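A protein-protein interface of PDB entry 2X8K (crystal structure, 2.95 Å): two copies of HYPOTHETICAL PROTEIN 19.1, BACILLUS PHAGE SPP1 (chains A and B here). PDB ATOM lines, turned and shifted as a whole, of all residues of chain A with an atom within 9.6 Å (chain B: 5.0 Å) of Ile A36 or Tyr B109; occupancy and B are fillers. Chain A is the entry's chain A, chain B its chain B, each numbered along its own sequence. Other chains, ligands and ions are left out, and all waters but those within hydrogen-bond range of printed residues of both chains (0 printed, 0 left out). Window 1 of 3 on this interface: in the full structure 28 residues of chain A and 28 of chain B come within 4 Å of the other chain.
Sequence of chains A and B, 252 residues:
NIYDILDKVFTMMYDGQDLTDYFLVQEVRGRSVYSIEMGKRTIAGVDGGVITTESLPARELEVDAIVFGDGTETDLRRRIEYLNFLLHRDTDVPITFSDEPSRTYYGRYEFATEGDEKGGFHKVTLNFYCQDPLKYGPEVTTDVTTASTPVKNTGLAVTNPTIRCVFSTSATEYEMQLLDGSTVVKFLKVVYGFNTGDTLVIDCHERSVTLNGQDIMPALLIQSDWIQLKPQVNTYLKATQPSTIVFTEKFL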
ATOM      1  N   SER A  32      11.238 -15.269   9.053  1.00  0.00           N
ATOM      2  CA  SER A  32      12.541 -15.368   8.458  1.00  0.00           C
ATOM      3  C   SER A  32      13.244 -16.395   9.334  1.00  0.00           C
ATOM      4  O   SER A  32      12.573 -17.181  10.041  1.00  0.00           O
ATOM      5  CB  SER A  32      13.279 -14.044   8.613  1.00  0.00           C
ATOM      6  OG  SER A  32      14.379 -13.871   7.732  1.00  0.00           O
ATOM      7  N   VAL A  33      14.589 -16.409   9.256  1.00  0.00           N
ATOM      8  CA  VAL A  33      15.433 -17.340   9.973  1.00  0.00           C
ATOM      9  C   VAL A  33      15.078 -17.410  11.444  1.00  0.00           C
ATOM     10  O   VAL A  33      15.232 -16.441  12.175  1.00  0.00           O
ATOM     11  CB  VAL A  33      16.937 -17.069   9.695  1.00  0.00           C
ATOM     12  CG1 VAL A  33      17.791 -18.235  10.179  1.00  0.00           C
ATOM     13  CG2 VAL A  33      17.185 -16.790   8.212  1.00  0.00           C
ATOM     14  N   TYR A  34      14.521 -18.534  11.850  1.00  0.00           N
ATOM     15  CA  TYR A  34      14.090 -18.735  13.231  1.00  0.00           C
ATOM     16  C   TYR A  34      15.257 -18.802  14.191  1.00  0.00           C
ATOM     17  O   TYR A  34      16.320 -19.303  13.814  1.00  0.00           O
ATOM     18  CB  TYR A  34      13.209 -19.980  13.349  1.00  0.00           C
ATOM     19  CG  TYR A  34      12.069 -19.775  14.316  1.00  0.00           C
ATOM     20  CD1 TYR A  34      10.928 -19.072  13.943  1.00  0.00           C
ATOM     21  CD2 TYR A  34      12.118 -20.306  15.602  1.00  0.00           C
ATOM     22  CE1 TYR A  34       9.875 -18.885  14.832  1.00  0.00           C
ATOM     23  CE2 TYR A  34      11.059 -20.155  16.488  1.00  0.00           C
ATOM     24  CZ  TYR A  34       9.945 -19.435  16.104  1.00  0.00           C
ATOM     25  OH  TYR A  34       8.915 -19.265  16.995  1.00  0.00           O
ATOM     26  N   SER A  35      15.081 -18.235  15.403  1.00  0.00           N
ATOM     27  CA  SER A  35      16.112 -18.234  16.440  1.00  0.00           C
ATOM     28  C   SER A  35      15.874 -19.385  17.404  1.00  0.00           C
ATOM     29  O   SER A  35      14.796 -19.971  17.359  1.00  0.00           O
ATOM     30  CB  SER A  35      16.102 -16.895  17.146  1.00  0.00           C
ATOM     31  OG  SER A  35      16.482 -15.894  16.212  1.00  0.00           O
ATOM     32  N   ILE A  36      16.871 -19.749  18.229  1.00  0.00           N
ATOM     33  CA  ILE A  36      16.775 -20.847  19.200  1.00  0.00           C
ATOM     34  C   ILE A  36      17.089 -20.399  20.627  1.00  0.00           C
ATOM     35  O   ILE A  36      18.090 -19.714  20.872  1.00  0.00           O
ATOM     36  CB  ILE A  36      17.692 -22.003  18.774  1.00  0.00           C
ATOM     37  CG1 ILE A  36      17.181 -22.674  17.501  1.00  0.00           C
ATOM     38  CG2 ILE A  36      17.867 -23.026  19.881  1.00  0.00           C
ATOM     39  CD1 ILE A  36      18.259 -22.970  16.546  1.00  0.00           C
ATOM     40  N   GLU A  37      16.238 -20.812  21.576  1.00  0.00           N
ATOM     41  CA  GLU A  37      16.474 -20.556  22.995  1.00  0.00           C
ATOM     42  C   GLU A  37      17.471 -21.633  23.479  1.00  0.00           C
ATOM     43  O   GLU A  37      17.228 -22.833  23.311  1.00  0.00           O
ATOM     44  CB  GLU A  37      15.172 -20.603  23.813  1.00  0.00           C
ATOM     45  CG  GLU A  37      14.224 -19.442  23.574  1.00  0.00           C
ATOM     46  CD  GLU A  37      14.738 -18.056  23.922  1.00  0.00           C
ATOM     47  OE1 GLU A  37      14.587 -17.134  23.082  1.00  0.00           O
ATOM     48  OE2 GLU A  37      15.282 -17.891  25.041  1.00  0.00           O
ATOM     49  N   MET A  38      18.607 -21.190  24.026  1.00  0.00           N
ATOM     50  CA  MET A  38      19.639 -22.072  24.538  1.00  0.00           C
ATOM     51  C   MET A  38      19.959 -21.743  25.976  1.00  0.00           C
ATOM     52  O   MET A  38      20.207 -20.577  26.298  1.00  0.00           O
ATOM     53  CB  MET A  38      20.915 -21.913  23.724  1.00  0.00           C
ATOM     54  CG  MET A  38      20.880 -22.649  22.457  1.00  0.00           C
ATOM     55  SD  MET A  38      22.506 -22.672  21.710  1.00  0.00           S
ATOM     56  CE  MET A  38      22.032 -23.140  20.064  1.00  0.00           C
ATOM     57  N   GLY A  39      20.000 -22.769  26.813  1.00  0.00           N
ATOM     58  CA  GLY A  39      20.373 -22.621  28.208  1.00  0.00           C
ATOM     59  C   GLY A  39      21.872 -22.746  28.318  1.00  0.00           C
ATOM     60  O   GLY A  39      22.407 -23.828  28.075  1.00  0.00           O
ATOM     61  N   LYS A  40      22.571 -21.642  28.616  1.00  0.00           N
ATOM     62  CA  LYS A  40      24.028 -21.685  28.726  1.00  0.00           C
ATOM     63  C   LYS A  40      24.442 -21.652  30.182  1.00  0.00           C
ATOM     64  O   LYS A  40      23.868 -20.885  30.951  1.00  0.00           O
ATOM     65  CB  LYS A  40      24.671 -20.506  27.992  1.00  0.00           C
ATOM     66  CG  LYS A  40      24.696 -20.626  26.478  1.00  0.00           C
ATOM     67  CD  LYS A  40      23.999 -19.414  25.899  1.00  0.00           C
ATOM     68  CE  LYS A  40      24.305 -19.124  24.467  1.00  0.00           C
ATOM     69  NZ  LYS A  40      23.787 -17.786  24.093  1.00  0.00           N
ATOM     70  N   ILE A  51      25.919 -25.789  26.712  1.00  0.00           N
ATOM     71  CA  ILE A  51      24.505 -25.738  26.368  1.00  0.00           C
ATOM     72  C   ILE A  51      23.841 -26.795  27.236  1.00  0.00           C
ATOM     73  O   ILE A  51      24.294 -27.945  27.282  1.00  0.00           O
ATOM     74  CB  ILE A  51      24.222 -25.886  24.854  1.00  0.00           C
ATOM     75  CG1 ILE A  51      24.904 -24.738  24.079  1.00  0.00           C
ATOM     76  CG2 ILE A  51      22.717 -25.860  24.586  1.00  0.00           C
ATOM     77  CD1 ILE A  51      25.440 -25.100  22.754  1.00  0.00           C
ATOM     78  N   THR A  53      20.139 -26.661  27.758  1.00  0.00           N
ATOM     79  CA  THR A  53      18.809 -26.824  27.173  1.00  0.00           C
ATOM     80  C   THR A  53      18.743 -26.128  25.827  1.00  0.00           C
ATOM     81  O   THR A  53      19.513 -25.207  25.571  1.00  0.00           O
ATOM     82  CB  THR A  53      17.708 -26.329  28.130  1.00  0.00           C
ATOM     83  OG1 THR A  53      18.132 -25.147  28.810  1.00  0.00           O
ATOM     84  CG2 THR A  53      17.285 -27.393  29.132  1.00  0.00           C
ATOM     85  N   GLU A  54      17.839 -26.576  24.959  1.00  0.00           N
ATOM     86  CA  GLU A  54      17.633 -26.023  23.623  1.00  0.00           C
ATOM     87  C   GLU A  54      16.160 -26.188  23.274  1.00  0.00           C
ATOM     88  O   GLU A  54      15.637 -27.296  23.350  1.00  0.00           O
ATOM     89  CB  GLU A  54      18.507 -26.765  22.610  1.00  0.00           C
ATOM     90  CG  GLU A  54      19.332 -25.882  21.707  1.00  0.00           C
ATOM     91  CD  GLU A  54      19.978 -26.627  20.561  1.00  0.00           C
ATOM     92  OE1 GLU A  54      19.242 -27.137  19.684  1.00  0.00           O
ATOM     93  OE2 GLU A  54      21.228 -26.678  20.529  1.00  0.00           O
ATOM     94  N   SER A  55      15.482 -25.095  22.925  1.00  0.00           N
ATOM     95  CA  SER A  55      14.071 -25.122  22.556  1.00  0.00           C
ATOM     96  C   SER A  55      13.735 -24.037  21.563  1.00  0.00           C
ATOM     97  O   SER A  55      14.366 -22.985  21.533  1.00  0.00           O
ATOM     98  CB  SER A  55      13.184 -24.981  23.791  1.00  0.00           C
ATOM     99  OG  SER A  55      13.619 -23.959  24.674  1.00  0.00           O
ATOM    100  N   LEU A  56      12.709 -24.272  20.780  1.00  0.00           N
ATOM    101  CA  LEU A  56      12.205 -23.298  19.825  1.00  0.00           C
ATOM    102  C   LEU A  56      11.307 -22.308  20.557  1.00  0.00           C
ATOM    103  O   LEU A  56      10.320 -22.704  21.177  1.00  0.00           O
ATOM    104  CB  LEU A  56      11.374 -24.026  18.771  1.00  0.00           C
ATOM    105  CG  LEU A  56      11.940 -24.176  17.369  1.00  0.00           C
ATOM    106  CD1 LEU A  56      13.486 -24.396  17.342  1.00  0.00           C
ATOM    107  CD2 LEU A  56      11.184 -25.251  16.657  1.00  0.00           C
ATOM    108  N   PRO A  57      11.593 -21.006  20.500  1.00  0.00           N
ATOM    109  CA  PRO A  57      10.676 -20.048  21.138  1.00  0.00           C
ATOM    110  C   PRO A  57       9.324 -19.986  20.402  1.00  0.00           C
ATOM    111  O   PRO A  57       9.196 -20.467  19.281  1.00  0.00           O
ATOM    112  CB  PRO A  57      11.425 -18.732  21.009  1.00  0.00           C
ATOM    113  CG  PRO A  57      12.248 -18.901  19.779  1.00  0.00           C
ATOM    114  CD  PRO A  57      12.697 -20.323  19.799  1.00  0.00           C
ATOM    115  N   ALA A  58       8.310 -19.399  21.037  1.00  0.00           N
ATOM    116  CA  ALA A  58       7.009 -19.199  20.404  1.00  0.00           C
ATOM    117  C   ALA A  58       7.204 -18.139  19.304  1.00  0.00           C
ATOM    118  O   ALA A  58       8.196 -17.406  19.341  1.00  0.00           O
ATOM    119  CB  ALA A  58       6.030 -18.699  21.426  1.00  0.00           C
ATOM    120  N   LEU A 252       9.613 -24.669   9.755  1.00  0.00           N
ATOM    121  CA  LEU A 252       9.916 -23.581  10.699  1.00  0.00           C
ATOM    122  C   LEU A 252       9.984 -22.179  10.000  1.00  0.00           C
ATOM    123  O   LEU A 252       9.479 -21.203  10.588  1.00  0.00           O
ATOM    124  CB  LEU A 252      11.223 -23.828  11.504  1.00  0.00           C
ATOM    125  CG  LEU A 252      11.159 -23.773  13.039  1.00  0.00           C
ATOM    126  CD1 LEU A 252      12.489 -23.518  13.603  1.00  0.00           C
ATOM    127  CD2 LEU A 252      10.211 -22.685  13.565  1.00  0.00           C
ATOM    128  OXT LEU A 252      10.612 -22.038   8.923  1.00  0.00           O
ATOM    129  N   TYR B  14      28.678 -25.636   7.195  1.00  0.00           N
ATOM    130  CA  TYR B  14      28.076 -25.889   8.502  1.00  0.00           C
ATOM    131  C   TYR B  14      27.576 -27.317   8.462  1.00  0.00           C
ATOM    132  O   TYR B  14      26.666 -27.603   7.695  1.00  0.00           O
ATOM    133  CB  TYR B  14      26.926 -24.908   8.734  1.00  0.00           C
ATOM    134  CG  TYR B  14      26.138 -25.085  10.013  1.00  0.00           C
ATOM    135  CD1 TYR B  14      26.637 -24.626  11.230  1.00  0.00           C
ATOM    136  CD2 TYR B  14      24.847 -25.612   9.993  1.00  0.00           C
ATOM    137  CE1 TYR B  14      25.896 -24.741  12.406  1.00  0.00           C
ATOM    138  CE2 TYR B  14      24.097 -25.736  11.163  1.00  0.00           C
ATOM    139  CZ  TYR B  14      24.625 -25.293  12.367  1.00  0.00           C
ATOM    140  OH  TYR B  14      23.895 -25.390  13.526  1.00  0.00           O
ATOM    141  N   LEU B  87      20.089 -25.162   9.380  1.00  0.00           N
ATOM    142  CA  LEU B  87      20.684 -24.530  10.538  1.00  0.00           C
ATOM    143  C   LEU B  87      20.364 -25.132  11.884  1.00  0.00           C
ATOM    144  O   LEU B  87      21.268 -25.186  12.706  1.00  0.00           O
ATOM    145  CB  LEU B  87      20.393 -23.023  10.556  1.00  0.00           C
ATOM    146  CG  LEU B  87      21.025 -22.180   9.466  1.00  0.00           C
ATOM    147  CD1 LEU B  87      20.316 -20.865   9.346  1.00  0.00           C
ATOM    148  CD2 LEU B  87      22.531 -21.989   9.693  1.00  0.00           C
ATOM    149  N   HIS B  88      19.100 -25.497  12.170  1.00  0.00           N
ATOM    150  CA  HIS B  88      18.735 -26.006  13.499  1.00  0.00           C
ATOM    151  C   HIS B  88      19.389 -27.340  13.796  1.00  0.00           C
ATOM    152  O   HIS B  88      19.158 -28.331  13.094  1.00  0.00           O
ATOM    153  CB  HIS B  88      17.210 -25.966  13.768  1.00  0.00           C
ATOM    154  CG  HIS B  88      16.765 -26.429  15.143  1.00  0.00           C
ATOM    155  ND1 HIS B  88      15.646 -27.236  15.302  1.00  0.00           N
ATOM    156  CD2 HIS B  88      17.271 -26.159  16.374  1.00  0.00           C
ATOM    157  CE1 HIS B  88      15.515 -27.428  16.611  1.00  0.00           C
ATOM    158  NE2 HIS B  88      16.472 -26.813  17.297  1.00  0.00           N
ATOM    159  N   GLY B 107      30.579 -25.650  16.808  1.00  0.00           N
ATOM    160  CA  GLY B 107      29.451 -24.948  17.398  1.00  0.00           C
ATOM    161  C   GLY B 107      28.171 -25.187  16.631  1.00  0.00           C
ATOM    162  O   GLY B 107      28.131 -26.015  15.710  1.00  0.00           O
ATOM    163  N   ARG B 108      27.101 -24.491  17.045  1.00  0.00           N
ATOM    164  CA  ARG B 108      25.817 -24.611  16.399  1.00  0.00           C
ATOM    165  C   ARG B 108      25.145 -23.303  16.292  1.00  0.00           C
ATOM    166  O   ARG B 108      25.358 -22.457  17.153  1.00  0.00           O
ATOM    167  CB  ARG B 108      24.917 -25.650  17.068  1.00  0.00           C
ATOM    168  CG  ARG B 108      24.444 -25.356  18.472  1.00  0.00           C
ATOM    169  CD  ARG B 108      24.961 -26.479  19.316  1.00  0.00           C
ATOM    170  NE  ARG B 108      23.953 -27.177  20.116  1.00  0.00           N
ATOM    171  CZ  ARG B 108      24.252 -28.114  21.018  1.00  0.00           C
ATOM    172  NH1 ARG B 108      25.514 -28.458  21.234  1.00  0.00           N
ATOM    173  NH2 ARG B 108      23.290 -28.712  21.706  1.00  0.00           N
ATOM    174  N   TYR B 109      24.330 -23.124  15.231  1.00  0.00           N
ATOM    175  CA  TYR B 109      23.557 -21.903  14.999  1.00  0.00           C
ATOM    176  C   TYR B 109      22.703 -21.583  16.232  1.00  0.00           C
ATOM    177  O   TYR B 109      22.154 -22.501  16.843  1.00  0.00           O
ATOM    178  CB  TYR B 109      22.688 -22.072  13.726  1.00  0.00           C
ATOM    179  CG  TYR B 109      21.577 -21.060  13.621  1.00  0.00           C
ATOM    180  CD1 TYR B 109      21.832 -19.760  13.203  1.00  0.00           C
ATOM    181  CD2 TYR B 109      20.289 -21.374  14.029  1.00  0.00           C
ATOM    182  CE1 TYR B 109      20.823 -18.800  13.178  1.00  0.00           C
ATOM    183  CE2 TYR B 109      19.279 -20.424  14.032  1.00  0.00           C
ATOM    184  CZ  TYR B 109      19.543 -19.142  13.589  1.00  0.00           C
ATOM    185  OH  TYR B 109      18.525 -18.223  13.524  1.00  0.00           O
ATOM    186  N   GLU B 110      22.571 -20.306  16.586  1.00  0.00           N
ATOM    187  CA  GLU B 110      21.780 -19.954  17.757  1.00  0.00           C
ATOM    188  C   GLU B 110      20.599 -19.048  17.451  1.00  0.00           C
ATOM    189  O   GLU B 110      19.491 -19.349  17.851  1.00  0.00           O
ATOM    190  CB  GLU B 110      22.663 -19.312  18.825  1.00  0.00           C
ATOM    191  CG  GLU B 110      21.957 -19.330  20.154  1.00  0.00           C
ATOM    192  CD  GLU B 110      22.453 -18.397  21.223  1.00  0.00           C
ATOM    193  OE1 GLU B 110      23.509 -17.751  21.025  1.00  0.00           O
ATOM    194  OE2 GLU B 110      21.784 -18.333  22.280  1.00  0.00           O
ATOM    195  N   PHE B 111      20.843 -17.902  16.825  1.00  0.00           N
ATOM    196  CA  PHE B 111      19.791 -16.940  16.561  1.00  0.00           C
ATOM    197  C   PHE B 111      20.164 -16.038  15.420  1.00  0.00           C
ATOM    198  O   PHE B 111      21.345 -15.830  15.135  1.00  0.00           O
ATOM    199  CB  PHE B 111      19.484 -16.123  17.827  1.00  0.00           C
ATOM    200  CG  PHE B 111      20.544 -15.131  18.219  1.00  0.00           C
ATOM    201  CD1 PHE B 111      21.607 -15.507  19.040  1.00  0.00           C
ATOM    202  CD2 PHE B 111      20.476 -13.807  17.790  1.00  0.00           C
ATOM    203  CE1 PHE B 111      22.593 -14.582  19.412  1.00  0.00           C
ATOM    204  CE2 PHE B 111      21.456 -12.883  18.168  1.00  0.00           C
ATOM    205  CZ  PHE B 111      22.505 -13.279  18.983  1.00  0.00           C
ATOM    206  N   ALA B 112      19.141 -15.490  14.781  1.00  0.00           N
ATOM    207  CA  ALA B 112      19.248 -14.541  13.691  1.00  0.00           C
ATOM    208  C   ALA B 112      18.655 -13.196  14.104  1.00  0.00           C
ATOM    209  O   ALA B 112      17.717 -13.146  14.908  1.00  0.00           O
ATOM    210  CB  ALA B 112      18.498 -15.073  12.478  1.00  0.00           C
ATOM    211  N   LEU B 126      23.498 -14.042  11.184  1.00  0.00           N
ATOM    212  CA  LEU B 126      23.335 -15.379  11.733  1.00  0.00           C
ATOM    213  C   LEU B 126      24.362 -15.500  12.843  1.00  0.00           C
ATOM    214  O   LEU B 126      25.535 -15.185  12.636  1.00  0.00           O
ATOM    215  CB  LEU B 126      23.529 -16.461  10.665  1.00  0.00           C
ATOM    216  CG  LEU B 126      22.603 -16.408   9.445  1.00  0.00           C
ATOM    217  CD1 LEU B 126      23.022 -17.435   8.416  1.00  0.00           C
ATOM    218  CD2 LEU B 126      21.157 -16.628   9.824  1.00  0.00           C
ATOM    219  N   ASN B 127      23.917 -15.897  14.036  1.00  0.00           N
ATOM    220  CA  ASN B 127      24.796 -16.014  15.194  1.00  0.00           C
ATOM    221  C   ASN B 127      24.964 -17.458  15.570  1.00  0.00           C
ATOM    222  O   ASN B 127      23.964 -18.135  15.836  1.00  0.00           O
ATOM    223  CB  ASN B 127      24.247 -15.205  16.356  1.00  0.00           C
ATOM    224  CG  ASN B 127      24.246 -13.734  16.086  1.00  0.00           C
ATOM    225  OD1 ASN B 127      23.335 -13.188  15.478  1.00  0.00           O
ATOM    226  ND2 ASN B 127      25.274 -13.065  16.522  1.00  0.00           N
ATOM    227  N   PHE B 128      26.231 -17.933  15.576  1.00  0.00           N
ATOM    228  CA  PHE B 128      26.624 -19.316  15.878  1.00  0.00           C
ATOM    229  C   PHE B 128      27.357 -19.367  17.194  1.00  0.00           C
ATOM    230  O   PHE B 128      28.292 -18.588  17.407  1.00  0.00           O
ATOM    231  CB  PHE B 128      27.521 -19.879  14.767  1.00  0.00           C
ATOM    232  CG  PHE B 128      26.873 -19.914  13.409  1.00  0.00           C
ATOM    233  CD1 PHE B 128      26.275 -21.076  12.937  1.00  0.00           C
ATOM    234  CD2 PHE B 128      26.840 -18.781  12.608  1.00  0.00           C
ATOM    235  CE1 PHE B 128      25.657 -21.103  11.686  1.00  0.00           C
ATOM    236  CE2 PHE B 128      26.210 -18.808  11.361  1.00  0.00           C
ATOM    237  CZ  PHE B 128      25.628 -19.972  10.906  1.00  0.00           C
ATOM    238  N   TYR B 129      26.964 -20.310  18.064  1.00  0.00           N
ATOM    239  CA  TYR B 129      27.541 -20.457  19.395  1.00  0.00           C
ATOM    240  C   TYR B 129      28.454 -21.616  19.473  1.00  0.00           C
ATOM    241  O   TYR B 129      28.047 -22.733  19.164  1.00  0.00           O
ATOM    242  CB  TYR B 129      26.432 -20.604  20.444  1.00  0.00           C
ATOM    243  CG  TYR B 129      26.927 -20.657  21.871  1.00  0.00           C
ATOM    244  CD1 TYR B 129      27.425 -19.520  22.503  1.00  0.00           C
ATOM    245  CD2 TYR B 129      26.836 -21.825  22.616  1.00  0.00           C
ATOM    246  CE1 TYR B 129      27.854 -19.557  23.830  1.00  0.00           C
ATOM    247  CE2 TYR B 129      27.264 -21.874  23.947  1.00  0.00           C
ATOM    248  CZ  TYR B 129      27.769 -20.736  24.553  1.00  0.00           C
ATOM    249  OH  TYR B 129      28.187 -20.770  25.865  1.00  0.00           O
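Of the printed residues of chain B, Tyr A34 touches Tyr B109. Of chain B, only His B88 (3.3 Å), Tyr B109 (3.6 Å) and Glu B110 (2.7 Å) come within 4 Å of Ile A36. Tyr B14 touches none of the printed residues of chain A. Of the printed residues of chain A, His B88 touches Ile A36, Glu A54 and Leu A56. Of the printed residues of chain A, Arg B108 touches Met A38, Ile A51 and Glu A54. Of chain A, only Val A33 (3.4 Å), Tyr A34 (2.5 Å), Ser A35 (3.8 Å), Ile A36 (3.6 Å) and Met A38 (3.3 Å) come within 4 Å of Tyr B109. Of the printed residues of chain A, Glu B110 touches Ser A35, Ile A36, Met A38 and Lys A40. Ala B112 touches just these residues of chain A: Val A33 (3.6 Å) and Ser A35 (3.0 Å). Of the printed residues of chain A, Tyr B129 touches Lys A40 and Ile A51. The nearest residue of chain A that does not touch Tyr B109 is Glu A54 (5.6 Å).
Of the 17 printed residues of chain A, 9 touch a printed residue of chain B. Hydrophobic or aromatic side chains of chain A that line the printed part of chain B: Val A33, Ile A36, Met A38, Ile A51 and Leu A56. Among the printed residues, 22 pairs touch across the chains. Among the printed residues, Asp or Glu carboxylates within 4 Å of a Lys or Arg side-chain nitrogen of the other chain: Lys A40 with Glu B110 (2.8 Å) and Glu A54 with Arg B108 (2.8 Å).
The side-chain hydroxyl (OH) of Tyr A34 lies within hydrogen-bond range of the backbone carbonyl oxygen (O) of Pro A57, 2.6 Å away. OH of Tyr A34 sits at hydrogen-bond distance from O of Ala A58, at 3.1 Å. The side-chain hydroxyl (OH) of Tyr B14 is in hydrogen-bond range of the backbone carbonyl oxygen (O) of Leu B87. N of Ala B112 sits at hydrogen-bond distance from OH of Tyr B109 (3.1 Å). The backbone carbonyl oxygen (O) of Asn B127 lies within hydrogen-bond range of the backbone NH (N) of Glu B110 (2.7 Å). O of Phe B111 is in hydrogen-bond range of N of Asn B127.
OH of Tyr B109 is in hydrogen-bond range of O of Tyr A34. The backbone NH (N) of Ala B112 lies within hydrogen-bond range of the side-chain hydroxyl (OG) of Ser A35, 3.0 Å away. The backbone carbonyl oxygen (O) of Glu B110 lies within hydrogen-bond range of the backbone NH (N) of Ile A36, at 2.7 Å. NZ of Lys A40 is in salt-bridge range of OE2 of Glu B110 (2.8 Å). The side-chain carboxylate (OE2) of Glu A54 is in salt-bridge range of the guanidinium group (NE) of Arg B108, 2.8 Å away.
No position is printed for both chains.
Among the printed residues, merely in contact across the chains: Met A38 with Tyr B109, Ile A36 with His B88, Ser A35 with Phe B111, Val A33 with Tyr B109, Lys A40 with Tyr B129, Val A33 with Ala B112, Ile A51 with Tyr B129, Ile A36 with Tyr B109, Met A38 with Arg B108, Ser A35 with Glu B110, Glu A54 with His B88, Ile A51 with Arg B108, Leu A56 with His B88, Met A38 with Glu B110, Val A33 with Leu B87, Val A33 with Leu B126 and Ser A35 with Tyr B109.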
